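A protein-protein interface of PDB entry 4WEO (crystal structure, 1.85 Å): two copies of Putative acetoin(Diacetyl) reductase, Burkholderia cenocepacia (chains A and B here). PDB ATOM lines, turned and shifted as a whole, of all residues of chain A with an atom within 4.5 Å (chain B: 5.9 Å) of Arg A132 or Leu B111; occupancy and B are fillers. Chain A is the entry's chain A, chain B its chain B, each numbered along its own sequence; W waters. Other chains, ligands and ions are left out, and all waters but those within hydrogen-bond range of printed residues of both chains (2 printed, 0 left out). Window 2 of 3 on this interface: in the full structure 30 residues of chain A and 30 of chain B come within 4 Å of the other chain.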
ATOM      1  N   ALA A  76      10.424   6.331  -4.955  1.00  0.00           N
ATOM      2  CA  ALA A  76      11.025   5.318  -4.083  1.00  0.00           C
ATOM      3  C   ALA A  76      12.542   5.150  -4.289  1.00  0.00           C
ATOM      4  O   ALA A  76      13.284   4.963  -3.323  1.00  0.00           O
ATOM      5  CB  ALA A  76      10.318   3.985  -4.276  1.00  0.00           C
ATOM      6  N   PHE A 128       5.254   7.189   3.861  1.00  0.00           N
ATOM      7  CA  PHE A 128       5.325   5.735   3.723  1.00  0.00           C
ATOM      8  C   PHE A 128       6.657   5.287   3.113  1.00  0.00           C
ATOM      9  O   PHE A 128       7.297   4.382   3.641  1.00  0.00           O
ATOM     10  CB  PHE A 128       4.145   5.223   2.871  1.00  0.00           C
ATOM     11  CG  PHE A 128       4.398   3.904   2.175  1.00  0.00           C
ATOM     12  CD1 PHE A 128       4.647   2.744   2.904  1.00  0.00           C
ATOM     13  CD2 PHE A 128       4.319   3.811   0.797  1.00  0.00           C
ATOM     14  CE1 PHE A 128       4.866   1.528   2.255  1.00  0.00           C
ATOM     15  CE2 PHE A 128       4.519   2.598   0.143  1.00  0.00           C
ATOM     16  CZ  PHE A 128       4.792   1.460   0.868  1.00  0.00           C
ATOM     17  N   LEU A 129       7.072   5.922   2.016  1.00  0.00           N
ATOM     18  CA  LEU A 129       8.290   5.535   1.324  1.00  0.00           C
ATOM     19  C   LEU A 129       9.529   5.777   2.174  1.00  0.00           C
ATOM     20  O   LEU A 129      10.470   4.983   2.142  1.00  0.00           O
ATOM     21  CB  LEU A 129       8.418   6.286   0.000  1.00  0.00           C
ATOM     22  CG  LEU A 129       7.430   5.868  -1.081  1.00  0.00           C
ATOM     23  CD1 LEU A 129       7.589   6.742  -2.322  1.00  0.00           C
ATOM     24  CD2 LEU A 129       7.628   4.381  -1.434  1.00  0.00           C
ATOM     25  N   GLY A 130       9.540   6.889   2.900  1.00  0.00           N
ATOM     26  CA  GLY A 130      10.655   7.206   3.768  1.00  0.00           C
ATOM     27  C   GLY A 130      10.779   6.187   4.878  1.00  0.00           C
ATOM     28  O   GLY A 130      11.855   5.650   5.120  1.00  0.00           O
ATOM     29  N   CYS A 131       9.662   5.913   5.545  1.00  0.00           N
ATOM     30  CA  CYS A 131       9.637   4.948   6.628  1.00  0.00           C
ATOM     31  C   CYS A 131      10.057   3.574   6.145  1.00  0.00           C
ATOM     32  O   CYS A 131      10.841   2.888   6.801  1.00  0.00           O
ATOM     33  CB  CYS A 131       8.242   4.874   7.250  1.00  0.00           C
ATOM     34  SG  CYS A 131       7.799   6.372   8.159  1.00  0.00           S
ATOM     35  N   ARG A 132       9.502   3.155   5.013  1.00  0.00           N
ATOM     36  CA  ARG A 132       9.802   1.831   4.494  1.00  0.00           C
ATOM     37  C   ARG A 132      11.288   1.693   4.183  1.00  0.00           C
ATOM     38  O   ARG A 132      11.890   0.642   4.434  1.00  0.00           O
ATOM     39  CB  ARG A 132       8.963   1.538   3.246  1.00  0.00           C
ATOM     40  CG  ARG A 132       9.079   0.100   2.746  1.00  0.00           C
ATOM     41  CD  ARG A 132       8.316  -0.108   1.437  1.00  0.00           C
ATOM     42  NE  ARG A 132       8.929   0.628   0.334  1.00  0.00           N
ATOM     43  CZ  ARG A 132       8.606   0.463  -0.946  1.00  0.00           C
ATOM     44  NH1 ARG A 132       7.665  -0.413  -1.290  1.00  0.00           N
ATOM     45  NH2 ARG A 132       9.224   1.175  -1.885  1.00  0.00           N
ATOM     46  N   ALA A 133      11.879   2.755   3.637  1.00  0.00           N
ATOM     47  CA  ALA A 133      13.284   2.718   3.226  1.00  0.00           C
ATOM     48  C   ALA A 133      14.236   2.617   4.415  1.00  0.00           C
ATOM     49  O   ALA A 133      15.313   2.039   4.298  1.00  0.00           O
ATOM     50  CB  ALA A 133      13.619   3.955   2.407  1.00  0.00           C
ATOM     51  N   ALA A 134      13.837   3.155   5.561  1.00  0.00           N
ATOM     52  CA  ALA A 134      14.736   3.191   6.710  1.00  0.00           C
ATOM     53  C   ALA A 134      14.545   1.985   7.623  1.00  0.00           C
ATOM     54  O   ALA A 134      15.361   1.719   8.503  1.00  0.00           O
ATOM     55  CB  ALA A 134      14.528   4.473   7.499  1.00  0.00           C
ATOM     56  N   LEU A 135      13.470   1.248   7.389  1.00  0.00           N
ATOM     57  CA  LEU A 135      13.027   0.207   8.309  1.00  0.00           C
ATOM     58  C   LEU A 135      14.048  -0.910   8.546  1.00  0.00           C
ATOM     59  O   LEU A 135      14.354  -1.235   9.704  1.00  0.00           O
ATOM     60  CB  LEU A 135      11.713  -0.379   7.782  1.00  0.00           C
ATOM     61  CG  LEU A 135      10.703  -1.009   8.716  1.00  0.00           C
ATOM     62  CD1 LEU A 135       9.365  -1.056   8.012  1.00  0.00           C
ATOM     63  CD2 LEU A 135      11.158  -2.407   9.115  1.00  0.00           C
ATOM     64  N   SER B 104      -5.653  -5.313   2.116  1.00  0.00           N
ATOM     65  CA  SER B 104      -4.646  -6.354   1.990  1.00  0.00           C
ATOM     66  C   SER B 104      -3.803  -6.308   3.251  1.00  0.00           C
ATOM     67  O   SER B 104      -3.767  -5.286   3.928  1.00  0.00           O
ATOM     68  CB  SER B 104      -3.782  -6.164   0.748  1.00  0.00           C
ATOM     69  OG  SER B 104      -3.028  -4.974   0.844  1.00  0.00           O
ATOM     70  N   ILE B 105      -3.131  -7.406   3.569  1.00  0.00           N
ATOM     71  CA  ILE B 105      -2.372  -7.467   4.810  1.00  0.00           C
ATOM     72  C   ILE B 105      -0.888  -7.675   4.526  1.00  0.00           C
ATOM     73  O   ILE B 105      -0.486  -8.710   3.990  1.00  0.00           O
ATOM     74  CB  ILE B 105      -2.906  -8.585   5.710  1.00  0.00           C
ATOM     75  CG1 ILE B 105      -4.411  -8.394   5.927  1.00  0.00           C
ATOM     76  CG2 ILE B 105      -2.156  -8.615   7.034  1.00  0.00           C
ATOM     77  CD1 ILE B 105      -5.054  -9.543   6.635  1.00  0.00           C
ATOM     78  N   HIS B 106      -0.092  -6.663   4.855  1.00  0.00           N
ATOM     79  CA  HIS B 106       1.354  -6.721   4.715  1.00  0.00           C
ATOM     80  C   HIS B 106       2.016  -5.810   5.732  1.00  0.00           C
ATOM     81  O   HIS B 106       1.590  -4.672   5.906  1.00  0.00           O
ATOM     82  CB  HIS B 106       1.804  -6.276   3.318  1.00  0.00           C
ATOM     83  CG  HIS B 106       1.125  -6.986   2.188  1.00  0.00           C
ATOM     84  ND1 HIS B 106       1.524  -8.226   1.738  1.00  0.00           N
ATOM     85  CD2 HIS B 106       0.088  -6.616   1.399  1.00  0.00           C
ATOM     86  CE1 HIS B 106       0.751  -8.599   0.733  1.00  0.00           C
ATOM     87  NE2 HIS B 106      -0.127  -7.638   0.506  1.00  0.00           N
ATOM     88  N   PRO B 107       3.091  -6.282   6.372  1.00  0.00           N
ATOM     89  CA  PRO B 107       3.915  -5.356   7.163  1.00  0.00           C
ATOM     90  C   PRO B 107       4.475  -4.281   6.251  1.00  0.00           C
ATOM     91  O   PRO B 107       4.673  -4.559   5.065  1.00  0.00           O
ATOM     92  CB  PRO B 107       5.055  -6.234   7.692  1.00  0.00           C
ATOM     93  CG  PRO B 107       4.664  -7.644   7.400  1.00  0.00           C
ATOM     94  CD  PRO B 107       3.678  -7.626   6.279  1.00  0.00           C
ATOM     95  N   VAL B 108       4.755  -3.101   6.790  1.00  0.00           N
ATOM     96  CA  VAL B 108       5.297  -1.997   6.000  1.00  0.00           C
ATOM     97  C   VAL B 108       6.570  -2.438   5.284  1.00  0.00           C
ATOM     98  O   VAL B 108       6.813  -2.067   4.130  1.00  0.00           O
ATOM     99  CB  VAL B 108       5.571  -0.759   6.894  1.00  0.00           C
ATOM    100  CG1 VAL B 108       6.379   0.300   6.149  1.00  0.00           C
ATOM    101  CG2 VAL B 108       4.250  -0.170   7.393  1.00  0.00           C
ATOM    102  N   ALA B 109       7.363  -3.272   5.951  1.00  0.00           N
ATOM    103  CA  ALA B 109       8.602  -3.763   5.354  1.00  0.00           C
ATOM    104  C   ALA B 109       8.337  -4.524   4.057  1.00  0.00           C
ATOM    105  O   ALA B 109       9.213  -4.632   3.206  1.00  0.00           O
ATOM    106  CB  ALA B 109       9.346  -4.647   6.337  1.00  0.00           C
ATOM    107  N   GLU B 110       7.132  -5.052   3.903  1.00  0.00           N
ATOM    108  CA  GLU B 110       6.809  -5.835   2.710  1.00  0.00           C
ATOM    109  C   GLU B 110       5.793  -5.180   1.782  1.00  0.00           C
ATOM    110  O   GLU B 110       5.485  -5.735   0.723  1.00  0.00           O
ATOM    111  CB  GLU B 110       6.319  -7.230   3.102  1.00  0.00           C
ATOM    112  CG  GLU B 110       7.359  -8.030   3.863  1.00  0.00           C
ATOM    113  CD  GLU B 110       6.933  -9.469   4.102  1.00  0.00           C
ATOM    114  OE1 GLU B 110       5.737  -9.790   3.920  1.00  0.00           O
ATOM    115  OE2 GLU B 110       7.819 -10.300   4.402  1.00  0.00           O
ATOM    116  N   LEU B 111       5.302  -4.001   2.154  1.00  0.00           N
ATOM    117  CA  LEU B 111       4.342  -3.270   1.324  1.00  0.00           C
ATOM    118  C   LEU B 111       4.966  -2.748   0.033  1.00  0.00           C
ATOM    119  O   LEU B 111       6.040  -2.159   0.054  1.00  0.00           O
ATOM    120  CB  LEU B 111       3.758  -2.086   2.094  1.00  0.00           C
ATOM    121  CG  LEU B 111       2.586  -2.357   3.027  1.00  0.00           C
ATOM    122  CD1 LEU B 111       2.235  -1.090   3.808  1.00  0.00           C
ATOM    123  CD2 LEU B 111       1.400  -2.830   2.193  1.00  0.00           C
ATOM    124  N   THR B 112       4.295  -2.984  -1.088  1.00  0.00           N
ATOM    125  CA  THR B 112       4.717  -2.408  -2.361  1.00  0.00           C
ATOM    126  C   THR B 112       3.996  -1.094  -2.608  1.00  0.00           C
ATOM    127  O   THR B 112       2.986  -0.796  -1.962  1.00  0.00           O
ATOM    128  CB  THR B 112       4.422  -3.346  -3.535  1.00  0.00           C
ATOM    129  OG1 THR B 112       3.006  -3.542  -3.613  1.00  0.00           O
ATOM    130  CG2 THR B 112       5.118  -4.704  -3.351  1.00  0.00           C
ATOM    131  N   GLU B 113       4.500  -0.317  -3.555  1.00  0.00           N
ATOM    132  CA  GLU B 113       3.786   0.875  -3.989  1.00  0.00           C
ATOM    133  C   GLU B 113       2.435   0.522  -4.575  1.00  0.00           C
ATOM    134  O   GLU B 113       1.480   1.276  -4.410  1.00  0.00           O
ATOM    135  CB  GLU B 113       4.580   1.661  -5.023  1.00  0.00           C
ATOM    136  CG  GLU B 113       5.654   2.535  -4.459  1.00  0.00           C
ATOM    137  CD  GLU B 113       6.265   3.401  -5.534  1.00  0.00           C
ATOM    138  OE1 GLU B 113       7.423   3.140  -5.917  1.00  0.00           O
ATOM    139  OE2 GLU B 113       5.572   4.337  -6.001  1.00  0.00           O
ATOM    140  N   ASP B 115       0.545  -1.911  -3.597  1.00  0.00           N
ATOM    141  CA  ASP B 115      -0.308  -2.157  -2.420  1.00  0.00           C
ATOM    142  C   ASP B 115      -0.850  -0.854  -1.831  1.00  0.00           C
ATOM    143  O   ASP B 115      -2.046  -0.714  -1.549  1.00  0.00           O
ATOM    144  CB  ASP B 115       0.463  -2.892  -1.306  1.00  0.00           C
ATOM    145  CG  ASP B 115       0.831  -4.322  -1.661  1.00  0.00           C
ATOM    146  OD1 ASP B 115       0.089  -4.974  -2.431  1.00  0.00           O
ATOM    147  OD2 ASP B 115       1.865  -4.804  -1.132  1.00  0.00           O
ATOM    148  N   TRP B 116       0.057   0.098  -1.649  1.00  0.00           N
ATOM    149  CA  TRP B 116      -0.285   1.389  -1.079  1.00  0.00           C
ATOM    150  C   TRP B 116      -1.295   2.114  -1.962  1.00  0.00           C
ATOM    151  O   TRP B 116      -2.340   2.567  -1.489  1.00  0.00           O
ATOM    152  CB  TRP B 116       0.975   2.252  -0.900  1.00  0.00           C
ATOM    153  CG  TRP B 116       0.665   3.644  -0.472  1.00  0.00           C
ATOM    154  CD1 TRP B 116       0.378   4.709  -1.281  1.00  0.00           C
ATOM    155  CD2 TRP B 116       0.591   4.128   0.869  1.00  0.00           C
ATOM    156  NE1 TRP B 116       0.128   5.825  -0.521  1.00  0.00           N
ATOM    157  CE2 TRP B 116       0.255   5.498   0.802  1.00  0.00           C
ATOM    158  CE3 TRP B 116       0.792   3.544   2.122  1.00  0.00           C
ATOM    159  CZ2 TRP B 116       0.115   6.289   1.939  1.00  0.00           C
ATOM    160  CZ3 TRP B 116       0.647   4.332   3.253  1.00  0.00           C
ATOM    161  CH2 TRP B 116       0.309   5.685   3.153  1.00  0.00           C
ATOM    162  N   ALA B 162      -0.956  -0.924   7.811  1.00  0.00           N
ATOM    163  CA  ALA B 162      -0.635   0.496   7.942  1.00  0.00           C
ATOM    164  C   ALA B 162      -1.180   1.307   6.770  1.00  0.00           C
ATOM    165  O   ALA B 162      -1.626   2.439   6.947  1.00  0.00           O
ATOM    166  CB  ALA B 162       0.863   0.689   8.061  1.00  0.00           C
ATOM    167  N   HIS B 163      -1.122   0.725   5.575  1.00  0.00           N
ATOM    168  CA  HIS B 163      -1.643   1.372   4.380  1.00  0.00           C
ATOM    169  C   HIS B 163      -3.165   1.446   4.424  1.00  0.00           C
ATOM    170  O   HIS B 163      -3.771   2.450   4.038  1.00  0.00           O
ATOM    171  CB  HIS B 163      -1.192   0.624   3.112  1.00  0.00           C
ATOM    172  CG  HIS B 163      -1.606  -0.823   3.064  1.00  0.00           C
ATOM    173  ND1 HIS B 163      -1.538  -1.663   4.155  1.00  0.00           N
ATOM    174  CD2 HIS B 163      -2.058  -1.584   2.039  1.00  0.00           C
ATOM    175  CE1 HIS B 163      -1.949  -2.872   3.812  1.00  0.00           C
ATOM    176  NE2 HIS B 163      -2.269  -2.852   2.529  1.00  0.00           N
HETATM  177  O   HOH W   1       7.972   6.073  -6.549  1.00  0.00           O
HETATM  178  O   HOH W   2       8.925   1.139  -4.762  1.00  0.00           O
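O of Leu B111 sits at hydrogen-bond distance from NH1 of Arg A132 (2.7 Å).
OG1 of Thr B112 lies within hydrogen-bond range of N of Asp B115 (3.0 Å).
Glu B113 touches Ala A76. CB of Leu B111 touches CE1 of Phe A128, 3.8 Å away. Phe A128 touches Trp B116. Arg A132 touches Val B108 (CG to O, 3.4 Å). Thr B112 touches Arg A132. Glu B113 touches Arg A132. Val B108 touches Leu A135. CD1 of Leu A135 touches N of Ala B109, at 3.6 Å.
Printed residues of chain B within 4 Å of Ala A76: Glu B113 (3.4 Å). Arg A132 touches four residues of chain B. Of the printed residues of chain B, Leu A135 touches Val B108 (3.8 Å) and Ala B109 (3.6 Å). His B106 touches none of the printed residues of chain A. Of the printed residues of chain A, Val B108 touches Arg A132 and Leu A135. Leu B111 touches just these residues of chain A: Phe A128 (3.8 Å) and Arg A132 (2.7 Å). Of the printed residues of chain A, Thr B112 touches Arg A132. Printed residues of chain A within 4 Å of Trp B116: Phe A128. The nearest printed residue of chain A that does not touch Leu B111 is Leu A129 (6.9 Å). The nearest printed residue of chain A that does not touch Ala B109 is Arg A132 (4.7 Å).
Of the 9 printed residues of chain A, 4 touch a printed residue of chain B. Hydrophobic or aromatic side chains of chain A within 4 Å of the printed part of chain B: Ala A76, Phe A128 and Leu A135. Along chain B the printed residues that touch a printed residue of chain A span positions 108 to 116. Among the printed residues, 9 pairs touch across the chains. Among the printed residues, no Asp or Glu carboxylate lies within 4 Å of a Lys or Arg side-chain nitrogen of the other chain.
No position is printed for both chains.
Water W2 bridges the side-chain carboxylate (OE1) of Glu B113 and the guanidinium group (NH2) of Arg A132. Water W1 lies within hydrogen-bond range of N of Ala A76 (2.9 Å) and OE2 of Glu B113 (3.0 Å).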
